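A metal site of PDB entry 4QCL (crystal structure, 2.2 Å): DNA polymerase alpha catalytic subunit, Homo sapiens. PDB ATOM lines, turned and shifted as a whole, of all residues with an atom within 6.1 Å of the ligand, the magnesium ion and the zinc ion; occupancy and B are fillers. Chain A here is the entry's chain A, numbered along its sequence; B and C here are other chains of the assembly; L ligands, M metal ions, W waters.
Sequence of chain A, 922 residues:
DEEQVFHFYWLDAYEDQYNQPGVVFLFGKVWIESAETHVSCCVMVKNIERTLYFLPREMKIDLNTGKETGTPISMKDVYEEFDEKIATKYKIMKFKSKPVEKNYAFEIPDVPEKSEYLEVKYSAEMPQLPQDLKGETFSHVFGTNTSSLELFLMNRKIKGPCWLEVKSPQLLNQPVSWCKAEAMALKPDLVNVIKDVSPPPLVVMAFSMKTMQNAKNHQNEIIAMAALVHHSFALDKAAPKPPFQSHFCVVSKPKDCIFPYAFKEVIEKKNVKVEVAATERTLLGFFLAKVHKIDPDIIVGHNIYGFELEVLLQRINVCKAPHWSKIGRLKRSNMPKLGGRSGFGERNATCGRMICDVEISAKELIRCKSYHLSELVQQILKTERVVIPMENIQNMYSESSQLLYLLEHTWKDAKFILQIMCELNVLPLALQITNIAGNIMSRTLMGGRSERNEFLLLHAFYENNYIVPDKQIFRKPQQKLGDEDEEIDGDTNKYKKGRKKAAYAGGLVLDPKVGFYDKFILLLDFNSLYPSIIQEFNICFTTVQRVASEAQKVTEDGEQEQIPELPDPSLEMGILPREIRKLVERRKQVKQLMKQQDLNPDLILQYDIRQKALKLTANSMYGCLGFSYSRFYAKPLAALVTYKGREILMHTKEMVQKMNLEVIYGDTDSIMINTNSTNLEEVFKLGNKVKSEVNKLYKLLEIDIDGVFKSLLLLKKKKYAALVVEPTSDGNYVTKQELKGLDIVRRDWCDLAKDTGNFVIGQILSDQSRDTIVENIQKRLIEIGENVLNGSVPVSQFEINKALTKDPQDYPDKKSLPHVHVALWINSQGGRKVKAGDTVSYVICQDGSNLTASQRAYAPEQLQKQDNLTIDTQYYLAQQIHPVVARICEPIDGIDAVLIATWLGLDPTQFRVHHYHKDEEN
The backbone NH of Ser 528 is in hydrogen-bond range of an oxygen (O12) of the ligand (2.8 Å).
The guanidinium group (NH2) of Arg 587 lies within salt-bridge range of an oxygen (O11) of the ligand (2.8 Å).
O6 of DG 10 of chain B lies within hydrogen-bond range of a nitrogen (N3) of the ligand, at 3.1 Å.
N of Tyr 530 sits at hydrogen-bond distance from O3 of the ligand (2.9 Å).
O6 of the ligand lies within salt-bridge range of NZ of Lys 615, 3.1 Å away.
N4 of DC 11 of chain C sits at hydrogen-bond distance from a nitrogen (N3) of the ligand.
The backbone NH of Leu 529 lies within hydrogen-bond range of an oxygen (O8) of the ligand (3.4 Å).
NH1 of Arg 587 is in hydrogen-bond range of OG of Ser 528 (3.3 Å).
The guanidinium group (NE) of Arg 587 is in hydrogen-bond range of the side-chain amide oxygen (OE1) of Gln 611, 2.5 Å away.
N7 of DG 10 of chain B sits close to the side-chain hydroxyl (OG) of Ser 620 (3.5 Å).
The side-chain carboxylate (OD1) of Asp 667 sits at hydrogen-bond distance from the side-chain hydroxyl (OG1) of Thr 668 (2.7 Å).
OG of Ser 620 lies within hydrogen-bond range of O of Leu 616, at 2.9 Å.
N2 of DG 11 of chain B sits close to an oxygen (O1) of the ligand (3.3 Å).
Asn 527 touches the ligand (CA to O12, 3.2 Å).
Pro 531 touches the ligand.
Leu 616 touches the ligand (CD2 to N3, 3.9 Å).
ND2 of Asn 619 touches C6 of the ligand, 3.8 Å away.
CE2 of Tyr 622 touches O1 of the ligand, 3.9 Å away.
Thr 668 touches the ligand (CG2 to O2, 3.9 Å).
Hydrophobic or aromatic side chains within 4 Å of the ligand: Leu 529, Tyr 530, Pro 531, Leu 616 and Tyr 622.
Of the 24 residues printed, 3 come within 4 Å of the magnesium ion.
DC 11 of chain C touches the zinc ion (C3' to ZN, 3.9 Å).
Of the 24 residues printed, 3 come within 4 Å of the zinc ion.
The magnesium ion is bound by O13 of the ligand, 1.8 Å away.
The magnesium ion is bound by O9 of the ligand (2.0 Å).
OD2 of Asp 525 is bound to the magnesium ion (2.0 Å).
The magnesium ion is bound by O of Phe 526, at 2.0 Å.
OD1 of Asp 669 binds the magnesium ion, at 2.1 Å.
The magnesium ion is bound by O5 of the ligand (2.3 Å).
The magnesium ion has six donor atoms within binding distance.
The zinc ion is bound by water W3 (1.9 Å), the side-chain carboxylate (OD2) of Asp 669 (1.9 Å), the side-chain carboxylate (OD1) of Asp 525 (2.0 Å), an oxygen (O5) of the ligand (2.4 Å) and water W9 (2.5 Å).
The zinc ion has five donor atoms within binding distance.
Water W9 bridges O of Asp 667 and OG of Ser 670.
Water W8 lies within hydrogen-bond range of O12 of the ligand, OD1 of Asn 527 and NZ of Lys 591.
Water W7 lies within hydrogen-bond range of an oxygen (O11) of the ligand and the guanidinium group of Arg 587.
Water W4 bridges the side-chain amide nitrogen of Asn 619 and an oxygen (O8) of the ligand.
Water W6 lies within hydrogen-bond range of the side-chain amide oxygen of Asn 619 (2.9 Å) and a nitrogen (N3) of the ligand (3.3 Å).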
ATOM      1  N   ASP A 525     -27.472 -20.173  -9.091  1.00  0.00           N
ATOM      2  CA  ASP A 525     -26.372 -19.580  -8.354  1.00  0.00           C
ATOM      3  C   ASP A 525     -26.568 -19.758  -6.831  1.00  0.00           C
ATOM      4  O   ASP A 525     -27.645 -19.507  -6.307  1.00  0.00           O
ATOM      5  CB  ASP A 525     -26.316 -18.092  -8.702  1.00  0.00           C
ATOM      6  CG  ASP A 525     -25.065 -17.404  -8.208  1.00  0.00           C
ATOM      7  OD1 ASP A 525     -24.214 -17.048  -9.063  1.00  0.00           O
ATOM      8  OD2 ASP A 525     -24.922 -17.232  -6.987  1.00  0.00           O
ATOM      9  N   PHE A 526     -25.517 -20.208  -6.123  1.00  0.00           N
ATOM     10  CA  PHE A 526     -25.578 -20.374  -4.668  1.00  0.00           C
ATOM     11  C   PHE A 526     -25.639 -19.022  -3.918  1.00  0.00           C
ATOM     12  O   PHE A 526     -24.942 -18.069  -4.295  1.00  0.00           O
ATOM     13  CB  PHE A 526     -24.333 -21.110  -4.164  1.00  0.00           C
ATOM     14  CG  PHE A 526     -24.375 -22.582  -4.366  1.00  0.00           C
ATOM     15  CD1 PHE A 526     -23.665 -23.173  -5.409  1.00  0.00           C
ATOM     16  CD2 PHE A 526     -25.101 -23.403  -3.501  1.00  0.00           C
ATOM     17  CE1 PHE A 526     -23.681 -24.551  -5.601  1.00  0.00           C
ATOM     18  CE2 PHE A 526     -25.128 -24.775  -3.681  1.00  0.00           C
ATOM     19  CZ  PHE A 526     -24.417 -25.355  -4.736  1.00  0.00           C
ATOM     20  N   ASN A 527     -26.452 -18.936  -2.872  1.00  0.00           N
ATOM     21  CA  ASN A 527     -26.565 -17.700  -2.069  1.00  0.00           C
ATOM     22  C   ASN A 527     -25.363 -17.613  -1.110  1.00  0.00           C
ATOM     23  O   ASN A 527     -25.060 -18.578  -0.406  1.00  0.00           O
ATOM     24  CB  ASN A 527     -27.848 -17.695  -1.211  1.00  0.00           C
ATOM     25  CG  ASN A 527     -29.131 -17.675  -2.040  1.00  0.00           C
ATOM     26  OD1 ASN A 527     -29.332 -16.808  -2.901  1.00  0.00           O
ATOM     27  ND2 ASN A 527     -30.018 -18.616  -1.752  1.00  0.00           N
ATOM     28  N   SER A 528     -24.687 -16.470  -1.094  1.00  0.00           N
ATOM     29  CA  SER A 528     -23.541 -16.300  -0.175  1.00  0.00           C
ATOM     30  C   SER A 528     -22.646 -17.534  -0.065  1.00  0.00           C
ATOM     31  O   SER A 528     -22.289 -17.941   1.048  1.00  0.00           O
ATOM     32  CB  SER A 528     -24.076 -15.948   1.225  1.00  0.00           C
ATOM     33  OG  SER A 528     -24.983 -14.844   1.128  1.00  0.00           O
ATOM     34  N   LEU A 529     -22.242 -18.095  -1.199  1.00  0.00           N
ATOM     35  CA  LEU A 529     -21.417 -19.311  -1.167  1.00  0.00           C
ATOM     36  C   LEU A 529     -20.308 -19.372  -0.118  1.00  0.00           C
ATOM     37  O   LEU A 529     -20.373 -20.185   0.803  1.00  0.00           O
ATOM     38  CB  LEU A 529     -20.811 -19.604  -2.544  1.00  0.00           C
ATOM     39  CG  LEU A 529     -20.099 -20.970  -2.583  1.00  0.00           C
ATOM     40  CD1 LEU A 529     -21.146 -22.079  -2.466  1.00  0.00           C
ATOM     41  CD2 LEU A 529     -19.332 -21.131  -3.877  1.00  0.00           C
ATOM     42  N   TYR A 530     -19.280 -18.533  -0.250  1.00  0.00           N
ATOM     43  CA  TYR A 530     -18.162 -18.570   0.688  1.00  0.00           C
ATOM     44  C   TYR A 530     -18.557 -18.357   2.148  1.00  0.00           C
ATOM     45  O   TYR A 530     -18.071 -19.075   3.036  1.00  0.00           O
ATOM     46  CB  TYR A 530     -17.090 -17.546   0.275  1.00  0.00           C
ATOM     47  CG  TYR A 530     -16.224 -18.013  -0.880  1.00  0.00           C
ATOM     48  CD1 TYR A 530     -16.664 -19.009  -1.766  1.00  0.00           C
ATOM     49  CD2 TYR A 530     -14.977 -17.424  -1.123  1.00  0.00           C
ATOM     50  CE1 TYR A 530     -15.897 -19.391  -2.878  1.00  0.00           C
ATOM     51  CE2 TYR A 530     -14.203 -17.791  -2.228  1.00  0.00           C
ATOM     52  CZ  TYR A 530     -14.667 -18.777  -3.099  1.00  0.00           C
ATOM     53  OH  TYR A 530     -13.920 -19.113  -4.202  1.00  0.00           O
ATOM     54  N   PRO A 531     -19.412 -17.353   2.430  1.00  0.00           N
ATOM     55  CA  PRO A 531     -19.816 -17.146   3.820  1.00  0.00           C
ATOM     56  C   PRO A 531     -20.535 -18.401   4.335  1.00  0.00           C
ATOM     57  O   PRO A 531     -20.354 -18.809   5.483  1.00  0.00           O
ATOM     58  CB  PRO A 531     -20.730 -15.933   3.728  1.00  0.00           C
ATOM     59  CG  PRO A 531     -20.035 -15.110   2.671  1.00  0.00           C
ATOM     60  CD  PRO A 531     -19.728 -16.160   1.620  1.00  0.00           C
ATOM     61  N   ARG A 587     -28.041  -9.002   5.412  1.00  0.00           N
ATOM     62  CA  ARG A 587     -28.249  -8.875   3.971  1.00  0.00           C
ATOM     63  C   ARG A 587     -29.610  -9.438   3.549  1.00  0.00           C
ATOM     64  O   ARG A 587     -30.288  -8.854   2.691  1.00  0.00           O
ATOM     65  CB  ARG A 587     -27.124  -9.581   3.216  1.00  0.00           C
ATOM     66  CG  ARG A 587     -27.110  -9.248   1.736  1.00  0.00           C
ATOM     67  CD  ARG A 587     -26.105 -10.084   0.980  1.00  0.00           C
ATOM     68  NE  ARG A 587     -26.402 -10.094  -0.447  1.00  0.00           N
ATOM     69  CZ  ARG A 587     -26.158 -11.125  -1.244  1.00  0.00           C
ATOM     70  NH1 ARG A 587     -25.608 -12.237  -0.759  1.00  0.00           N
ATOM     71  NH2 ARG A 587     -26.491 -11.060  -2.527  1.00  0.00           N
ATOM     72  N   LYS A 591     -32.863  -7.777   1.600  1.00  0.00           N
ATOM     73  CA  LYS A 591     -33.382  -8.349   0.363  1.00  0.00           C
ATOM     74  C   LYS A 591     -34.874  -8.583   0.529  1.00  0.00           C
ATOM     75  O   LYS A 591     -35.636  -8.474  -0.429  1.00  0.00           O
ATOM     76  CB  LYS A 591     -32.650  -9.646   0.004  1.00  0.00           C
ATOM     77  CG  LYS A 591     -31.149  -9.441  -0.180  1.00  0.00           C
ATOM     78  CD  LYS A 591     -30.470 -10.593  -0.884  1.00  0.00           C
ATOM     79  CE  LYS A 591     -30.747 -10.549  -2.377  1.00  0.00           C
ATOM     80  NZ  LYS A 591     -29.911 -11.540  -3.105  1.00  0.00           N
ATOM     81  N   GLN A 611     -27.558  -3.792  -0.028  1.00  0.00           N
ATOM     82  CA  GLN A 611     -27.508  -5.257  -0.057  1.00  0.00           C
ATOM     83  C   GLN A 611     -26.148  -5.733  -0.607  1.00  0.00           C
ATOM     84  O   GLN A 611     -25.578  -6.710  -0.139  1.00  0.00           O
ATOM     85  CB  GLN A 611     -28.668  -5.771  -0.916  1.00  0.00           C
ATOM     86  CG  GLN A 611     -28.678  -7.248  -1.136  1.00  0.00           C
ATOM     87  CD  GLN A 611     -27.862  -7.652  -2.341  1.00  0.00           C
ATOM     88  OE1 GLN A 611     -27.124  -8.642  -2.291  1.00  0.00           O
ATOM     89  NE2 GLN A 611     -28.004  -6.918  -3.436  1.00  0.00           N
ATOM     90  N   LYS A 615     -22.804  -7.658   1.078  1.00  0.00           N
ATOM     91  CA  LYS A 615     -22.279  -8.844   0.420  1.00  0.00           C
ATOM     92  C   LYS A 615     -20.749  -8.701   0.364  1.00  0.00           C
ATOM     93  O   LYS A 615     -20.002  -9.610   0.733  1.00  0.00           O
ATOM     94  CB  LYS A 615     -22.866  -8.948  -1.000  1.00  0.00           C
ATOM     95  CG  LYS A 615     -22.219 -10.008  -1.867  1.00  0.00           C
ATOM     96  CD  LYS A 615     -22.920 -10.091  -3.208  1.00  0.00           C
ATOM     97  CE  LYS A 615     -22.160 -11.015  -4.157  1.00  0.00           C
ATOM     98  NZ  LYS A 615     -22.928 -11.198  -5.434  1.00  0.00           N
ATOM     99  N   LEU A 616     -20.301  -7.529  -0.067  1.00  0.00           N
ATOM    100  CA  LEU A 616     -18.888  -7.234  -0.170  1.00  0.00           C
ATOM    101  C   LEU A 616     -18.200  -7.304   1.178  1.00  0.00           C
ATOM    102  O   LEU A 616     -17.035  -7.709   1.263  1.00  0.00           O
ATOM    103  CB  LEU A 616     -18.691  -5.859  -0.788  1.00  0.00           C
ATOM    104  CG  LEU A 616     -18.542  -5.931  -2.311  1.00  0.00           C
ATOM    105  CD1 LEU A 616     -18.939  -4.597  -2.976  1.00  0.00           C
ATOM    106  CD2 LEU A 616     -17.099  -6.313  -2.616  1.00  0.00           C
ATOM    107  N   ASN A 619     -17.742 -10.995   1.987  1.00  0.00           N
ATOM    108  CA  ASN A 619     -16.708 -11.581   1.141  1.00  0.00           C
ATOM    109  C   ASN A 619     -15.333 -11.035   1.479  1.00  0.00           C
ATOM    110  O   ASN A 619     -14.324 -11.741   1.339  1.00  0.00           O
ATOM    111  CB  ASN A 619     -17.028 -11.401  -0.342  1.00  0.00           C
ATOM    112  CG  ASN A 619     -18.219 -12.248  -0.763  1.00  0.00           C
ATOM    113  OD1 ASN A 619     -18.857 -11.996  -1.797  1.00  0.00           O
ATOM    114  ND2 ASN A 619     -18.517 -13.264   0.033  1.00  0.00           N
ATOM    115  N   SER A 620     -15.276  -9.797   1.955  1.00  0.00           N
ATOM    116  CA  SER A 620     -14.006  -9.203   2.365  1.00  0.00           C
ATOM    117  C   SER A 620     -13.516  -9.875   3.642  1.00  0.00           C
ATOM    118  O   SER A 620     -12.323  -9.911   3.912  1.00  0.00           O
ATOM    119  CB  SER A 620     -14.143  -7.700   2.609  1.00  0.00           C
ATOM    120  OG  SER A 620     -14.248  -6.983   1.392  1.00  0.00           O
ATOM    121  N   TYR A 622     -13.794 -12.987   4.163  1.00  0.00           N
ATOM    122  CA  TYR A 622     -13.127 -14.196   3.681  1.00  0.00           C
ATOM    123  C   TYR A 622     -11.764 -13.781   3.101  1.00  0.00           C
ATOM    124  O   TYR A 622     -10.737 -14.388   3.401  1.00  0.00           O
ATOM    125  CB  TYR A 622     -13.949 -14.900   2.596  1.00  0.00           C
ATOM    126  CG  TYR A 622     -13.097 -15.453   1.479  1.00  0.00           C
ATOM    127  CD1 TYR A 622     -12.212 -16.520   1.702  1.00  0.00           C
ATOM    128  CD2 TYR A 622     -13.060 -14.821   0.239  1.00  0.00           C
ATOM    129  CE1 TYR A 622     -11.318 -16.935   0.709  1.00  0.00           C
ATOM    130  CE2 TYR A 622     -12.162 -15.222  -0.758  1.00  0.00           C
ATOM    131  CZ  TYR A 622     -11.293 -16.274  -0.523  1.00  0.00           C
ATOM    132  OH  TYR A 622     -10.400 -16.633  -1.504  1.00  0.00           O
ATOM    133  N   GLY A 623     -11.772 -12.721   2.305  1.00  0.00           N
ATOM    134  CA  GLY A 623     -10.562 -12.240   1.651  1.00  0.00           C
ATOM    135  C   GLY A 623      -9.420 -11.824   2.551  1.00  0.00           C
ATOM    136  O   GLY A 623      -8.255 -12.048   2.220  1.00  0.00           O
ATOM    137  N   ASP A 667     -19.562 -20.396 -13.265  1.00  0.00           N
ATOM    138  CA  ASP A 667     -18.474 -19.600 -12.704  1.00  0.00           C
ATOM    139  C   ASP A 667     -18.431 -19.574 -11.171  1.00  0.00           C
ATOM    140  O   ASP A 667     -19.187 -18.859 -10.524  1.00  0.00           O
ATOM    141  CB  ASP A 667     -18.574 -18.164 -13.243  1.00  0.00           C
ATOM    142  CG  ASP A 667     -17.399 -17.268 -12.795  1.00  0.00           C
ATOM    143  OD1 ASP A 667     -16.627 -17.655 -11.878  1.00  0.00           O
ATOM    144  OD2 ASP A 667     -17.275 -16.145 -13.353  1.00  0.00           O
ATOM    145  N   THR A 668     -17.516 -20.357 -10.605  1.00  0.00           N
ATOM    146  CA  THR A 668     -17.323 -20.402  -9.152  1.00  0.00           C
ATOM    147  C   THR A 668     -18.479 -20.986  -8.328  1.00  0.00           C
ATOM    148  O   THR A 668     -18.282 -21.936  -7.567  1.00  0.00           O
ATOM    149  CB  THR A 668     -16.997 -18.987  -8.586  1.00  0.00           C
ATOM    150  OG1 THR A 668     -15.944 -18.400  -9.363  1.00  0.00           O
ATOM    151  CG2 THR A 668     -16.540 -19.074  -7.112  1.00  0.00           C
ATOM    152  N   ASP A 669     -19.684 -20.422  -8.459  1.00  0.00           N
ATOM    153  CA  ASP A 669     -20.833 -20.902  -7.695  1.00  0.00           C
ATOM    154  C   ASP A 669     -22.092 -20.892  -8.539  1.00  0.00           C
ATOM    155  O   ASP A 669     -23.197 -20.768  -8.009  1.00  0.00           O
ATOM    156  CB  ASP A 669     -21.086 -20.034  -6.450  1.00  0.00           C
ATOM    157  CG  ASP A 669     -21.783 -18.713  -6.774  1.00  0.00           C
ATOM    158  OD1 ASP A 669     -22.747 -18.353  -6.067  1.00  0.00           O
ATOM    159  OD2 ASP A 669     -21.364 -18.009  -7.718  1.00  0.00           O
ATOM    160  N   SER A 670     -21.926 -20.995  -9.852  1.00  0.00           N
ATOM    161  CA  SER A 670     -23.075 -20.996 -10.734  1.00  0.00           C
ATOM    162  C   SER A 670     -23.041 -22.154 -11.749  1.00  0.00           C
ATOM    163  O   SER A 670     -21.997 -22.766 -11.987  1.00  0.00           O
ATOM    164  CB  SER A 670     -23.169 -19.652 -11.459  1.00  0.00           C
ATOM    165  OG  SER A 670     -22.055 -19.452 -12.295  1.00  0.00           O
ATOM    166  N   ASP A 706     -31.029 -17.966 -10.389  1.00  0.00           N
ATOM    167  CA  ASP A 706     -30.524 -16.611 -10.519  1.00  0.00           C
ATOM    168  C   ASP A 706     -31.297 -15.925 -11.640  1.00  0.00           C
ATOM    169  O   ASP A 706     -31.616 -14.734 -11.539  1.00  0.00           O
ATOM    170  CB  ASP A 706     -29.027 -16.649 -10.841  1.00  0.00           C
ATOM    171  CG  ASP A 706     -28.374 -15.290 -10.738  1.00  0.00           C
ATOM    172  OD1 ASP A 706     -28.438 -14.687  -9.647  1.00  0.00           O
ATOM    173  OD2 ASP A 706     -27.798 -14.821 -11.748  1.00  0.00           O
ATOM    174  P    DG B  10      -8.304  -2.903   1.558  1.00  0.00           P
ATOM    175  OP1  DG B  10      -9.409  -2.839   0.560  1.00  0.00           O
ATOM    176  OP2  DG B  10      -8.471  -2.281   2.893  1.00  0.00           O
ATOM    177  O5'  DG B  10      -7.969  -4.438   1.811  1.00  0.00           O
ATOM    178  C5'  DG B  10      -7.802  -5.313   0.716  1.00  0.00           C
ATOM    179  C4'  DG B  10      -8.104  -6.724   1.147  1.00  0.00           C
ATOM    180  O4'  DG B  10      -9.505  -6.806   1.463  1.00  0.00           O
ATOM    181  C3'  DG B  10      -7.885  -7.765   0.054  1.00  0.00           C
ATOM    182  O3'  DG B  10      -6.602  -8.356   0.201  1.00  0.00           O
ATOM    183  C2'  DG B  10      -8.915  -8.825   0.400  1.00  0.00           C
ATOM    184  C1'  DG B  10     -10.049  -8.049   1.031  1.00  0.00           C
ATOM    185  N9   DG B  10     -11.037  -7.709   0.000  1.00  0.00           N
ATOM    186  C8   DG B  10     -11.356  -6.454  -0.453  1.00  0.00           C
ATOM    187  N7   DG B  10     -12.239  -6.475  -1.411  1.00  0.00           N
ATOM    188  C5   DG B  10     -12.537  -7.820  -1.588  1.00  0.00           C
ATOM    189  C6   DG B  10     -13.432  -8.456  -2.476  1.00  0.00           C
ATOM    190  O6   DG B  10     -14.184  -7.944  -3.314  1.00  0.00           O
ATOM    191  N1   DG B  10     -13.400  -9.836  -2.325  1.00  0.00           N
ATOM    192  C2   DG B  10     -12.618 -10.511  -1.437  1.00  0.00           C
ATOM    193  N2   DG B  10     -12.723 -11.853  -1.456  1.00  0.00           N
ATOM    194  N3   DG B  10     -11.786  -9.943  -0.595  1.00  0.00           N
ATOM    195  C4   DG B  10     -11.794  -8.597  -0.726  1.00  0.00           C
ATOM    196  P    DG B  11      -5.830  -8.819  -1.118  1.00  0.00           P
ATOM    197  OP1  DG B  11      -4.406  -9.037  -0.754  1.00  0.00           O
ATOM    198  OP2  DG B  11      -6.177  -7.865  -2.206  1.00  0.00           O
ATOM    199  O5'  DG B  11      -6.518 -10.202  -1.459  1.00  0.00           O
ATOM    200  C5'  DG B  11      -6.431 -11.297  -0.553  1.00  0.00           C
ATOM    201  C4'  DG B  11      -7.128 -12.499  -1.129  1.00  0.00           C
ATOM    202  O4'  DG B  11      -8.536 -12.199  -1.218  1.00  0.00           O
ATOM    203  C3'  DG B  11      -6.693 -12.837  -2.559  1.00  0.00           C
ATOM    204  O3'  DG B  11      -5.749 -13.913  -2.549  1.00  0.00           O
ATOM    205  C2'  DG B  11      -7.965 -13.438  -3.155  1.00  0.00           C
ATOM    206  C1'  DG B  11      -9.108 -12.797  -2.374  1.00  0.00           C
ATOM    207  N9   DG B  11      -9.778 -11.743  -3.121  1.00  0.00           N
ATOM    208  C8   DG B  11      -9.509 -10.394  -3.094  1.00  0.00           C
ATOM    209  N7   DG B  11     -10.271  -9.706  -3.906  1.00  0.00           N
ATOM    210  C5   DG B  11     -11.103 -10.651  -4.488  1.00  0.00           C
ATOM    211  C6   DG B  11     -12.141 -10.506  -5.444  1.00  0.00           C
ATOM    212  O6   DG B  11     -12.553  -9.470  -5.983  1.00  0.00           O
ATOM    213  N1   DG B  11     -12.706 -11.735  -5.778  1.00  0.00           N
ATOM    214  C2   DG B  11     -12.335 -12.950  -5.251  1.00  0.00           C
ATOM    215  N2   DG B  11     -13.007 -14.023  -5.698  1.00  0.00           N
ATOM    216  N3   DG B  11     -11.384 -13.097  -4.346  1.00  0.00           N
ATOM    217  C4   DG B  11     -10.807 -11.918  -4.017  1.00  0.00           C
ATOM    218  P    DC C  11     -20.269 -11.676 -12.609  1.00  0.00           P
ATOM    219  OP1  DC C  11     -21.552 -12.190 -13.143  1.00  0.00           O
ATOM    220  OP2  DC C  11     -20.225 -10.319 -12.023  1.00  0.00           O
ATOM    221  O5'  DC C  11     -19.669 -12.703 -11.544  1.00  0.00           O
ATOM    222  C5'  DC C  11     -19.459 -14.046 -11.917  1.00  0.00           C
ATOM    223  C4'  DC C  11     -18.534 -14.747 -10.958  1.00  0.00           C
ATOM    224  O4'  DC C  11     -17.262 -14.070 -10.897  1.00  0.00           O
ATOM    225  C3'  DC C  11     -19.024 -14.776  -9.518  1.00  0.00           C
ATOM    226  C2'  DC C  11     -17.739 -14.887  -8.716  1.00  0.00           C
ATOM    227  C1'  DC C  11     -16.692 -14.226  -9.609  1.00  0.00           C
ATOM    228  N1   DC C  11     -16.248 -12.910  -9.120  1.00  0.00           N
ATOM    229  C2   DC C  11     -15.184 -12.863  -8.245  1.00  0.00           C
ATOM    230  O2   DC C  11     -14.624 -13.929  -7.937  1.00  0.00           O
ATOM    231  N3   DC C  11     -14.771 -11.665  -7.750  1.00  0.00           N
ATOM    232  C4   DC C  11     -15.394 -10.544  -8.123  1.00  0.00           C
ATOM    233  N4   DC C  11     -14.943  -9.393  -7.621  1.00  0.00           N
ATOM    234  C5   DC C  11     -16.498 -10.556  -9.026  1.00  0.00           C
ATOM    235  C6   DC C  11     -16.881 -11.749  -9.497  1.00  0.00           C
HETATM  236  N1  LIG L   1     -16.402 -13.519  -4.390  1.00  0.00           N
HETATM  237  C1  LIG L   1     -15.498 -12.726  -3.719  1.00  0.00           C
HETATM  238  N2  LIG L   1     -15.494 -11.385  -3.893  1.00  0.00           N
HETATM  239  C2  LIG L   1     -16.364 -10.788  -4.745  1.00  0.00           C
HETATM  240  C3  LIG L   1     -17.304 -11.567  -5.462  1.00  0.00           C
HETATM  241  C4  LIG L   1     -17.304 -12.928  -5.275  1.00  0.00           C
HETATM  242  O1  LIG L   1     -14.698 -13.225  -2.927  1.00  0.00           O
HETATM  243  N3  LIG L   1     -16.338  -9.424  -4.919  1.00  0.00           N
HETATM  244  C5  LIG L   1     -16.413 -14.998  -4.171  1.00  0.00           C
HETATM  245  C6  LIG L   1     -17.079 -15.245  -2.817  1.00  0.00           C
HETATM  246  C7  LIG L   1     -18.537 -15.542  -3.194  1.00  0.00           C
HETATM  247  C8  LIG L   1     -18.335 -16.405  -4.478  1.00  0.00           C
HETATM  248  O2  LIG L   1     -17.205 -15.718  -5.156  1.00  0.00           O
HETATM  249  O3  LIG L   1     -19.151 -16.323  -2.145  1.00  0.00           O
HETATM  250  C9  LIG L   1     -19.574 -16.375  -5.404  1.00  0.00           C
HETATM  251  O4  LIG L   1     -19.688 -15.107  -6.028  1.00  0.00           O
HETATM  252  P1  LIG L   1     -21.190 -14.491  -5.986  1.00  0.00           P
HETATM  253  O5  LIG L   1     -22.217 -15.510  -6.359  1.00  0.00           O
HETATM  254  O6  LIG L   1     -21.301 -13.275  -6.989  1.00  0.00           O
HETATM  255  O7  LIG L   1     -21.354 -13.896  -4.480  1.00  0.00           O
HETATM  256  P2  LIG L   1     -22.220 -14.741  -3.407  1.00  0.00           P
HETATM  257  O8  LIG L   1     -21.449 -14.917  -2.178  1.00  0.00           O
HETATM  258  O9  LIG L   1     -22.665 -16.182  -3.948  1.00  0.00           O
HETATM  259  O10 LIG L   1     -23.494 -13.763  -3.116  1.00  0.00           O
HETATM  260  P3  LIG L   1     -24.866 -14.081  -3.889  1.00  0.00           P
HETATM  261  O11 LIG L   1     -25.374 -12.813  -4.431  1.00  0.00           O
HETATM  262  O12 LIG L   1     -25.879 -14.697  -2.835  1.00  0.00           O
HETATM  263  O13 LIG L   1     -24.674 -15.117  -5.122  1.00  0.00           O
HETATM  264 MG    MG M   1     -23.884 -16.730  -5.372  1.00  0.00          MG
HETATM  265 ZN    ZN M   2     -22.321 -16.543  -8.551  1.00  0.00          ZN
HETATM  266  O   HOH W   1     -20.161 -10.734  -7.737  1.00  0.00           O
HETATM  267  O   HOH W   2     -24.624 -13.581  -7.568  1.00  0.00           O
HETATM  268  O   HOH W   3     -22.830 -14.861  -9.190  1.00  0.00           O
HETATM  269  O   HOH W   4     -21.372 -13.393   0.360  1.00  0.00           O
HETATM  270  O   HOH W   5     -18.576  -8.709  -6.290  1.00  0.00           O
HETATM  271  O   HOH W   6     -18.899  -9.359  -2.901  1.00  0.00           O
HETATM  272  O   HOH W   7     -27.263 -11.533  -5.890  1.00  0.00           O
HETATM  273  O   HOH W   8     -28.386 -14.168  -2.391  1.00  0.00           O
HETATM  274  O   HOH W   9     -20.947 -16.835 -10.599  1.00  0.00           O
